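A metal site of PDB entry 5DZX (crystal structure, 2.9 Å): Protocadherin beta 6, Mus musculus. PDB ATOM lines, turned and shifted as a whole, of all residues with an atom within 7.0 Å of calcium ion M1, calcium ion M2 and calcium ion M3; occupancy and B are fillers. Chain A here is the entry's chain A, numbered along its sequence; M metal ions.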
ATOM      1  N   GLU A 225       8.168 -18.965 -33.406  1.00  0.00           N
ATOM      2  CA  GLU A 225       9.394 -18.648 -34.124  1.00  0.00           C
ATOM      3  C   GLU A 225      10.147 -19.902 -34.564  1.00  0.00           C
ATOM      4  O   GLU A 225      11.142 -19.829 -35.285  1.00  0.00           O
ATOM      5  CB  GLU A 225      10.315 -17.777 -33.261  1.00  0.00           C
ATOM      6  CG  GLU A 225      10.788 -18.449 -31.981  1.00  0.00           C
ATOM      7  CD  GLU A 225      11.853 -17.643 -31.263  1.00  0.00           C
ATOM      8  OE1 GLU A 225      12.288 -18.076 -30.178  1.00  0.00           O
ATOM      9  OE2 GLU A 225      12.258 -16.581 -31.778  1.00  0.00           O
ATOM     10  N   LEU A 278      12.101 -18.367 -38.469  1.00  0.00           N
ATOM     11  CA  LEU A 278      11.738 -17.134 -37.776  1.00  0.00           C
ATOM     12  C   LEU A 278      12.521 -16.953 -36.478  1.00  0.00           C
ATOM     13  O   LEU A 278      13.210 -17.873 -36.030  1.00  0.00           O
ATOM     14  CB  LEU A 278      10.253 -17.096 -37.473  1.00  0.00           C
ATOM     15  CG  LEU A 278       9.318 -16.893 -38.665  1.00  0.00           C
ATOM     16  CD1 LEU A 278       7.875 -16.959 -38.219  1.00  0.00           C
ATOM     17  CD2 LEU A 278       9.622 -15.557 -39.314  1.00  0.00           C
ATOM     18  N   ASP A 279      12.403 -15.770 -35.899  1.00  0.00           N
ATOM     19  CA  ASP A 279      13.043 -15.458 -34.633  1.00  0.00           C
ATOM     20  C   ASP A 279      12.381 -14.251 -33.978  1.00  0.00           C
ATOM     21  O   ASP A 279      12.321 -13.173 -34.573  1.00  0.00           O
ATOM     22  CB  ASP A 279      14.538 -15.205 -34.823  1.00  0.00           C
ATOM     23  CG  ASP A 279      15.279 -15.113 -33.508  1.00  0.00           C
ATOM     24  OD1 ASP A 279      15.781 -16.152 -33.035  1.00  0.00           O
ATOM     25  OD2 ASP A 279      15.359 -13.999 -32.931  1.00  0.00           O
ATOM     26  N   PHE A 280      11.880 -14.445 -32.760  1.00  0.00           N
ATOM     27  CA  PHE A 280      11.173 -13.398 -32.036  1.00  0.00           C
ATOM     28  C   PHE A 280      12.128 -12.284 -31.624  1.00  0.00           C
ATOM     29  O   PHE A 280      11.734 -11.118 -31.532  1.00  0.00           O
ATOM     30  CB  PHE A 280      10.480 -13.984 -30.805  1.00  0.00           C
ATOM     31  CG  PHE A 280       9.530 -13.030 -30.129  1.00  0.00           C
ATOM     32  CD1 PHE A 280       9.963 -12.157 -29.153  1.00  0.00           C
ATOM     33  CD2 PHE A 280       8.181 -13.029 -30.461  1.00  0.00           C
ATOM     34  CE1 PHE A 280       9.083 -11.281 -28.530  1.00  0.00           C
ATOM     35  CE2 PHE A 280       7.301 -12.152 -29.838  1.00  0.00           C
ATOM     36  CZ  PHE A 280       7.754 -11.283 -28.873  1.00  0.00           C
ATOM     37  N   GLU A 281      13.379 -12.638 -31.362  1.00  0.00           N
ATOM     38  CA  GLU A 281      14.372 -11.675 -30.921  1.00  0.00           C
ATOM     39  C   GLU A 281      14.757 -10.719 -32.045  1.00  0.00           C
ATOM     40  O   GLU A 281      15.116  -9.561 -31.806  1.00  0.00           O
ATOM     41  CB  GLU A 281      15.618 -12.379 -30.364  1.00  0.00           C
ATOM     42  CG  GLU A 281      15.411 -13.095 -29.029  1.00  0.00           C
ATOM     43  CD  GLU A 281      14.583 -14.362 -29.152  1.00  0.00           C
ATOM     44  OE1 GLU A 281      14.531 -14.940 -30.254  1.00  0.00           O
ATOM     45  OE2 GLU A 281      13.990 -14.783 -28.139  1.00  0.00           O
ATOM     46  N   ALA A 282      14.684 -11.200 -33.278  1.00  0.00           N
ATOM     47  CA  ALA A 282      15.022 -10.378 -34.439  1.00  0.00           C
ATOM     48  C   ALA A 282      13.847  -9.516 -34.868  1.00  0.00           C
ATOM     49  O   ALA A 282      13.905  -8.290 -34.810  1.00  0.00           O
ATOM     50  CB  ALA A 282      15.481 -11.265 -35.601  1.00  0.00           C
ATOM     51  N   LEU A 309       5.240 -15.502 -31.831  1.00  0.00           N
ATOM     52  CA  LEU A 309       5.166 -15.784 -30.402  1.00  0.00           C
ATOM     53  C   LEU A 309       6.523 -16.210 -29.875  1.00  0.00           C
ATOM     54  O   LEU A 309       7.179 -17.073 -30.454  1.00  0.00           O
ATOM     55  CB  LEU A 309       4.122 -16.866 -30.126  1.00  0.00           C
ATOM     56  CG  LEU A 309       2.711 -16.534 -30.617  1.00  0.00           C
ATOM     57  CD1 LEU A 309       1.752 -17.679 -30.322  1.00  0.00           C
ATOM     58  CD2 LEU A 309       2.214 -15.246 -29.985  1.00  0.00           C
ATOM     59  N   ASP A 310       6.951 -15.587 -28.782  1.00  0.00           N
ATOM     60  CA  ASP A 310       8.260 -15.866 -28.206  1.00  0.00           C
ATOM     61  C   ASP A 310       8.310 -17.223 -27.516  1.00  0.00           C
ATOM     62  O   ASP A 310       7.559 -17.479 -26.575  1.00  0.00           O
ATOM     63  CB  ASP A 310       8.660 -14.784 -27.215  1.00  0.00           C
ATOM     64  CG  ASP A 310       9.949 -15.113 -26.484  1.00  0.00           C
ATOM     65  OD1 ASP A 310      11.037 -14.800 -27.011  1.00  0.00           O
ATOM     66  OD2 ASP A 310       9.881 -15.673 -25.368  1.00  0.00           O
ATOM     67  N   VAL A 311       9.183 -18.090 -28.006  1.00  0.00           N
ATOM     68  CA  VAL A 311       9.403 -19.381 -27.363  1.00  0.00           C
ATOM     69  C   VAL A 311      10.703 -19.325 -26.580  1.00  0.00           C
ATOM     70  O   VAL A 311      11.716 -18.828 -27.078  1.00  0.00           O
ATOM     71  CB  VAL A 311       9.452 -20.527 -28.406  1.00  0.00           C
ATOM     72  CG1 VAL A 311       9.738 -21.858 -27.721  1.00  0.00           C
ATOM     73  CG2 VAL A 311       8.143 -20.586 -29.184  1.00  0.00           C
ATOM     74  N   ASN A 312      10.685 -19.815 -25.344  1.00  0.00           N
ATOM     75  CA  ASN A 312      11.864 -19.774 -24.486  1.00  0.00           C
ATOM     76  C   ASN A 312      12.933 -20.739 -24.999  1.00  0.00           C
ATOM     77  O   ASN A 312      13.155 -21.801 -24.412  1.00  0.00           O
ATOM     78  CB  ASN A 312      11.485 -20.113 -23.043  1.00  0.00           C
ATOM     79  CG  ASN A 312      12.617 -19.850 -22.068  1.00  0.00           C
ATOM     80  OD1 ASN A 312      13.465 -18.998 -22.299  1.00  0.00           O
ATOM     81  ND2 ASN A 312      12.635 -20.594 -20.965  1.00  0.00           N
ATOM     82  N   ASP A 313      13.581 -20.364 -26.091  1.00  0.00           N
ATOM     83  CA  ASP A 313      14.579 -21.203 -26.741  1.00  0.00           C
ATOM     84  C   ASP A 313      16.001 -20.860 -26.323  1.00  0.00           C
ATOM     85  O   ASP A 313      16.939 -21.586 -26.645  1.00  0.00           O
ATOM     86  CB  ASP A 313      14.457 -21.069 -28.256  1.00  0.00           C
ATOM     87  CG  ASP A 313      14.706 -19.646 -28.745  1.00  0.00           C
ATOM     88  OD1 ASP A 313      14.508 -18.706 -27.945  1.00  0.00           O
ATOM     89  OD2 ASP A 313      15.120 -19.463 -29.910  1.00  0.00           O
ATOM     90  N   ASN A 314      16.159 -19.742 -25.619  1.00  0.00           N
ATOM     91  CA  ASN A 314      17.479 -19.304 -25.188  1.00  0.00           C
ATOM     92  C   ASN A 314      17.678 -19.353 -23.676  1.00  0.00           C
ATOM     93  O   ASN A 314      16.909 -18.769 -22.913  1.00  0.00           O
ATOM     94  CB  ASN A 314      17.747 -17.885 -25.688  1.00  0.00           C
ATOM     95  CG  ASN A 314      17.654 -17.785 -27.197  1.00  0.00           C
ATOM     96  OD1 ASN A 314      16.953 -16.928 -27.742  1.00  0.00           O
ATOM     97  ND2 ASN A 314      18.367 -18.667 -27.893  1.00  0.00           N
ATOM     98  N   ALA A 315      18.722 -20.054 -23.241  1.00  0.00           N
ATOM     99  CA  ALA A 315      19.035 -20.162 -21.821  1.00  0.00           C
ATOM    100  C   ALA A 315      19.826 -18.948 -21.333  1.00  0.00           C
ATOM    101  O   ALA A 315      20.598 -18.355 -22.097  1.00  0.00           O
ATOM    102  CB  ALA A 315      19.814 -21.450 -21.547  1.00  0.00           C
ATOM    103  N   PRO A 316      19.618 -18.552 -20.065  1.00  0.00           N
ATOM    104  CA  PRO A 316      20.324 -17.463 -19.393  1.00  0.00           C
ATOM    105  C   PRO A 316      21.840 -17.517 -19.597  1.00  0.00           C
ATOM    106  O   PRO A 316      22.414 -18.599 -19.626  1.00  0.00           O
ATOM    107  CB  PRO A 316      19.990 -17.690 -17.910  1.00  0.00           C
ATOM    108  CG  PRO A 316      18.732 -18.511 -17.899  1.00  0.00           C
ATOM    109  CD  PRO A 316      18.450 -19.019 -19.284  1.00  0.00           C
ATOM    110  N   ASP A 343      19.475 -12.403 -20.756  1.00  0.00           N
ATOM    111  CA  ASP A 343      18.546 -13.330 -21.390  1.00  0.00           C
ATOM    112  C   ASP A 343      17.842 -12.636 -22.551  1.00  0.00           C
ATOM    113  O   ASP A 343      17.082 -11.698 -22.332  1.00  0.00           O
ATOM    114  CB  ASP A 343      17.520 -13.854 -20.377  1.00  0.00           C
ATOM    115  CG  ASP A 343      16.827 -15.127 -20.842  1.00  0.00           C
ATOM    116  OD1 ASP A 343      16.906 -15.464 -22.044  1.00  0.00           O
ATOM    117  OD2 ASP A 343      16.180 -15.791 -20.000  1.00  0.00           O
ATOM    118  N   PRO A 344      18.101 -13.085 -23.790  1.00  0.00           N
ATOM    119  CA  PRO A 344      17.555 -12.446 -24.988  1.00  0.00           C
ATOM    120  C   PRO A 344      16.044 -12.618 -25.168  1.00  0.00           C
ATOM    121  O   PRO A 344      15.412 -11.806 -25.847  1.00  0.00           O
ATOM    122  CB  PRO A 344      18.307 -13.148 -26.124  1.00  0.00           C
ATOM    123  CG  PRO A 344      18.669 -14.470 -25.569  1.00  0.00           C
ATOM    124  CD  PRO A 344      18.978 -14.226 -24.121  1.00  0.00           C
ATOM    125  N   ASP A 345      15.478 -13.665 -24.565  1.00  0.00           N
ATOM    126  CA  ASP A 345      14.050 -13.939 -24.675  1.00  0.00           C
ATOM    127  C   ASP A 345      13.188 -12.832 -24.082  1.00  0.00           C
ATOM    128  O   ASP A 345      13.669 -12.012 -23.298  1.00  0.00           O
ATOM    129  CB  ASP A 345      13.713 -15.268 -23.994  1.00  0.00           C
ATOM    130  CG  ASP A 345      14.383 -16.460 -24.666  1.00  0.00           C
ATOM    131  OD1 ASP A 345      14.446 -16.482 -25.903  1.00  0.00           O
ATOM    132  OD2 ASP A 345      14.849 -17.359 -23.929  1.00  0.00           O
ATOM    133  N   SER A 346      11.912 -12.804 -24.460  1.00  0.00           N
ATOM    134  CA  SER A 346      10.980 -11.785 -23.973  1.00  0.00           C
ATOM    135  C   SER A 346      10.015 -12.368 -22.938  1.00  0.00           C
ATOM    136  O   SER A 346       9.922 -13.582 -22.787  1.00  0.00           O
ATOM    137  CB  SER A 346      10.201 -11.174 -25.145  1.00  0.00           C
ATOM    138  OG  SER A 346      11.074 -10.512 -26.043  1.00  0.00           O
ATOM    139  N   ASP A 348       8.376 -13.554 -19.449  1.00  0.00           N
ATOM    140  CA  ASP A 348       8.946 -14.242 -18.300  1.00  0.00           C
ATOM    141  C   ASP A 348      10.004 -15.242 -18.735  1.00  0.00           C
ATOM    142  O   ASP A 348      10.648 -15.883 -17.914  1.00  0.00           O
ATOM    143  CB  ASP A 348       7.850 -14.945 -17.486  1.00  0.00           C
ATOM    144  CG  ASP A 348       6.924 -13.980 -16.767  1.00  0.00           C
ATOM    145  OD1 ASP A 348       7.234 -12.773 -16.734  1.00  0.00           O
ATOM    146  OD2 ASP A 348       5.892 -14.435 -16.235  1.00  0.00           O
ATOM    147  N   ASN A 349      10.174 -15.380 -20.046  1.00  0.00           N
ATOM    148  CA  ASN A 349      11.222 -16.220 -20.597  1.00  0.00           C
ATOM    149  C   ASN A 349      12.574 -15.503 -20.500  1.00  0.00           C
ATOM    150  O   ASN A 349      13.627 -16.133 -20.543  1.00  0.00           O
ATOM    151  CB  ASN A 349      10.924 -16.597 -22.048  1.00  0.00           C
ATOM    152  CG  ASN A 349       9.572 -17.271 -22.217  1.00  0.00           C
ATOM    153  OD1 ASN A 349       9.157 -18.058 -21.374  1.00  0.00           O
ATOM    154  ND2 ASN A 349       8.895 -16.968 -23.312  1.00  0.00           N
ATOM    155  N   GLY A 350      12.514 -14.187 -20.360  1.00  0.00           N
ATOM    156  CA  GLY A 350      13.709 -13.366 -20.275  1.00  0.00           C
ATOM    157  C   GLY A 350      13.965 -12.814 -18.886  1.00  0.00           C
ATOM    158  O   GLY A 350      14.955 -12.104 -18.659  1.00  0.00           O
ATOM    159  N   ARG A 351      13.086 -13.128 -17.947  1.00  0.00           N
ATOM    160  CA  ARG A 351      13.269 -12.743 -16.555  1.00  0.00           C
ATOM    161  C   ARG A 351      14.049 -13.842 -15.852  1.00  0.00           C
ATOM    162  O   ARG A 351      13.716 -15.023 -15.965  1.00  0.00           O
ATOM    163  CB  ARG A 351      11.940 -12.510 -15.848  1.00  0.00           C
ATOM    164  CG  ARG A 351      11.189 -11.264 -16.279  1.00  0.00           C
ATOM    165  CD  ARG A 351       9.813 -11.204 -15.632  1.00  0.00           C
ATOM    166  NE  ARG A 351       9.890 -11.185 -14.176  1.00  0.00           N
ATOM    167  CZ  ARG A 351       8.836 -11.287 -13.370  1.00  0.00           C
ATOM    168  NH1 ARG A 351       8.997 -11.256 -12.049  1.00  0.00           N
ATOM    169  NH2 ARG A 351       7.623 -11.411 -13.876  1.00  0.00           N
ATOM    170  N   MET A 352      15.088 -13.466 -15.117  1.00  0.00           N
ATOM    171  CA  MET A 352      15.964 -14.440 -14.501  1.00  0.00           C
ATOM    172  C   MET A 352      16.032 -14.284 -12.996  1.00  0.00           C
ATOM    173  O   MET A 352      15.928 -13.174 -12.459  1.00  0.00           O
ATOM    174  CB  MET A 352      17.369 -14.344 -15.088  1.00  0.00           C
ATOM    175  CG  MET A 352      17.459 -14.648 -16.568  1.00  0.00           C
ATOM    176  SD  MET A 352      19.032 -14.089 -17.260  1.00  0.00           S
ATOM    177  CE  MET A 352      18.824 -12.308 -17.137  1.00  0.00           C
ATOM    178  N   ASP A 396      15.786 -18.913 -15.706  1.00  0.00           N
ATOM    179  CA  ASP A 396      14.707 -18.037 -16.112  1.00  0.00           C
ATOM    180  C   ASP A 396      13.370 -18.530 -15.556  1.00  0.00           C
ATOM    181  O   ASP A 396      13.296 -19.628 -15.008  1.00  0.00           O
ATOM    182  CB  ASP A 396      14.636 -17.919 -17.635  1.00  0.00           C
ATOM    183  CG  ASP A 396      14.638 -19.276 -18.325  1.00  0.00           C
ATOM    184  OD1 ASP A 396      14.363 -20.292 -17.656  1.00  0.00           O
ATOM    185  OD2 ASP A 396      14.888 -19.310 -19.548  1.00  0.00           O
ATOM    186  N   LEU A 397      12.328 -17.739 -15.735  1.00  0.00           N
ATOM    187  CA  LEU A 397      10.998 -18.094 -15.245  1.00  0.00           C
ATOM    188  C   LEU A 397      10.081 -18.526 -16.372  1.00  0.00           C
ATOM    189  O   LEU A 397       8.853 -18.439 -16.263  1.00  0.00           O
ATOM    190  CB  LEU A 397      10.388 -16.909 -14.481  1.00  0.00           C
ATOM    191  CG  LEU A 397      11.221 -16.404 -13.305  1.00  0.00           C
ATOM    192  CD1 LEU A 397      10.599 -15.145 -12.712  1.00  0.00           C
ATOM    193  CD2 LEU A 397      11.349 -17.487 -12.248  1.00  0.00           C
ATOM    194  N   GLY A 398      10.678 -19.005 -17.466  1.00  0.00           N
ATOM    195  CA  GLY A 398       9.914 -19.409 -18.628  1.00  0.00           C
ATOM    196  C   GLY A 398       9.344 -20.812 -18.541  1.00  0.00           C
ATOM    197  O   GLY A 398       9.485 -21.489 -17.516  1.00  0.00           O
ATOM    198  N   PRO A 400       9.427 -24.340 -20.817  1.00  0.00           N
ATOM    199  CA  PRO A 400      10.010 -24.800 -19.553  1.00  0.00           C
ATOM    200  C   PRO A 400      11.111 -23.870 -19.037  1.00  0.00           C
ATOM    201  O   PRO A 400      11.435 -22.892 -19.712  1.00  0.00           O
ATOM    202  CB  PRO A 400      10.607 -26.173 -19.916  1.00  0.00           C
ATOM    203  CG  PRO A 400       9.979 -26.537 -21.234  1.00  0.00           C
ATOM    204  CD  PRO A 400       9.763 -25.238 -21.926  1.00  0.00           C
ATOM    205  N   LEU A 402      14.858 -22.817 -18.240  1.00  0.00           N
ATOM    206  CA  LEU A 402      16.224 -23.077 -18.687  1.00  0.00           C
ATOM    207  C   LEU A 402      17.235 -22.606 -17.643  1.00  0.00           C
ATOM    208  O   LEU A 402      17.101 -21.506 -17.099  1.00  0.00           O
ATOM    209  CB  LEU A 402      16.495 -22.406 -20.025  1.00  0.00           C
ATOM    210  CG  LEU A 402      15.598 -22.848 -21.187  1.00  0.00           C
ATOM    211  CD1 LEU A 402      15.821 -21.987 -22.407  1.00  0.00           C
ATOM    212  CD2 LEU A 402      15.815 -24.315 -21.501  1.00  0.00           C
HETATM  213 CA    CA M   1      12.685 -16.878 -27.979  1.00  0.00          CA
HETATM  214 CA    CA M   2      15.040 -17.268 -30.935  1.00  0.00          CA
HETATM  215 CA    CA M   3      15.187 -17.553 -21.652  1.00  0.00          CA
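The side-chain amide nitrogen of Asn 312 sits at hydrogen-bond distance from the backbone carbonyl oxygen of Pro 400 (2.9 Å).
The side-chain carboxylate (OD2) of Asp 310 lies within hydrogen-bond range of the side-chain amide nitrogen (ND2) of Asn 349 (2.6 Å).
OD1 of Asp 313 lies close to OD1 of Asn 314 (3.0 Å).
The backbone NH of Ala 282 is in hydrogen-bond range of the side-chain carboxylate of Asp 279 (2.9 Å).
The side-chain carboxylate (OD1) of Asp 396 lies within hydrogen-bond range of the backbone NH (N) of Leu 402 (2.6 Å).
The side-chain carboxylate (OD1) of Asp 310 sits close to the backbone NH (N) of Ser 346 (3.4 Å).
Of the 28 residues printed, 6 come within 4 Å of calcium ion M1.
Of the 28 residues printed, 5 come within 4 Å of calcium ion M2.
The nearest printed residue that does not touch calcium ion M2 is Phe 280 (4.6 Å).
Along chain A the residues within 4 Å of calcium ion M3 span positions 312 to 396.
The nearest printed residue that does not touch calcium ion M3 is Pro 316 (4.3 Å).
Calcium ion M1 is bound by the backbone carbonyl oxygen (O) of Val 311 (2.4 Å), the side-chain carboxylate (OE2) of Glu 281 (2.5 Å), the side-chain carboxylate (OE1) of Glu 225 (2.5 Å), the side-chain carboxylate (OD1) of Asp 313 (2.6 Å), the side-chain carboxylate (OD1) of Asp 345 (2.8 Å) and the side-chain carboxylate (OD1) of Asp 310 (2.8 Å).
Calcium ion M2 is bound by the side-chain carboxylate (OD2) of Asp 313 (2.4 Å), the side-chain carboxylate (OE1) of Glu 281 (2.5 Å) and the side-chain carboxylate (OD1) of Asp 279 (2.5 Å).
Calcium ion M2 has three donor atoms within binding distance.
Slightly farther from calcium ion M2 lies the side-chain carboxylate (OE1) of Glu 225 (3.0 Å).
Slightly farther from calcium ion M2 lies the side-chain carboxylate (OE2) of Glu 225 (3.0 Å).
Calcium ion M3 is bound by OD2 of Asp 345, 2.3 Å away.
Calcium ion M3 is bound by the side-chain amide oxygen (OD1) of Asn 312.
Calcium ion M3 is bound by O of Asn 349 (2.4 Å).
Calcium ion M3 is bound by the backbone carbonyl oxygen (O) of Asn 314, at 2.5 Å.
The side-chain carboxylate (OD2) of Asp 343 binds calcium ion M3, 2.6 Å away.
Calcium ion M3 is bound by OD1 of Asp 343 (2.7 Å).
Calcium ion M3 is bound by the side-chain carboxylate (OD2) of Asp 396, at 2.8 Å.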
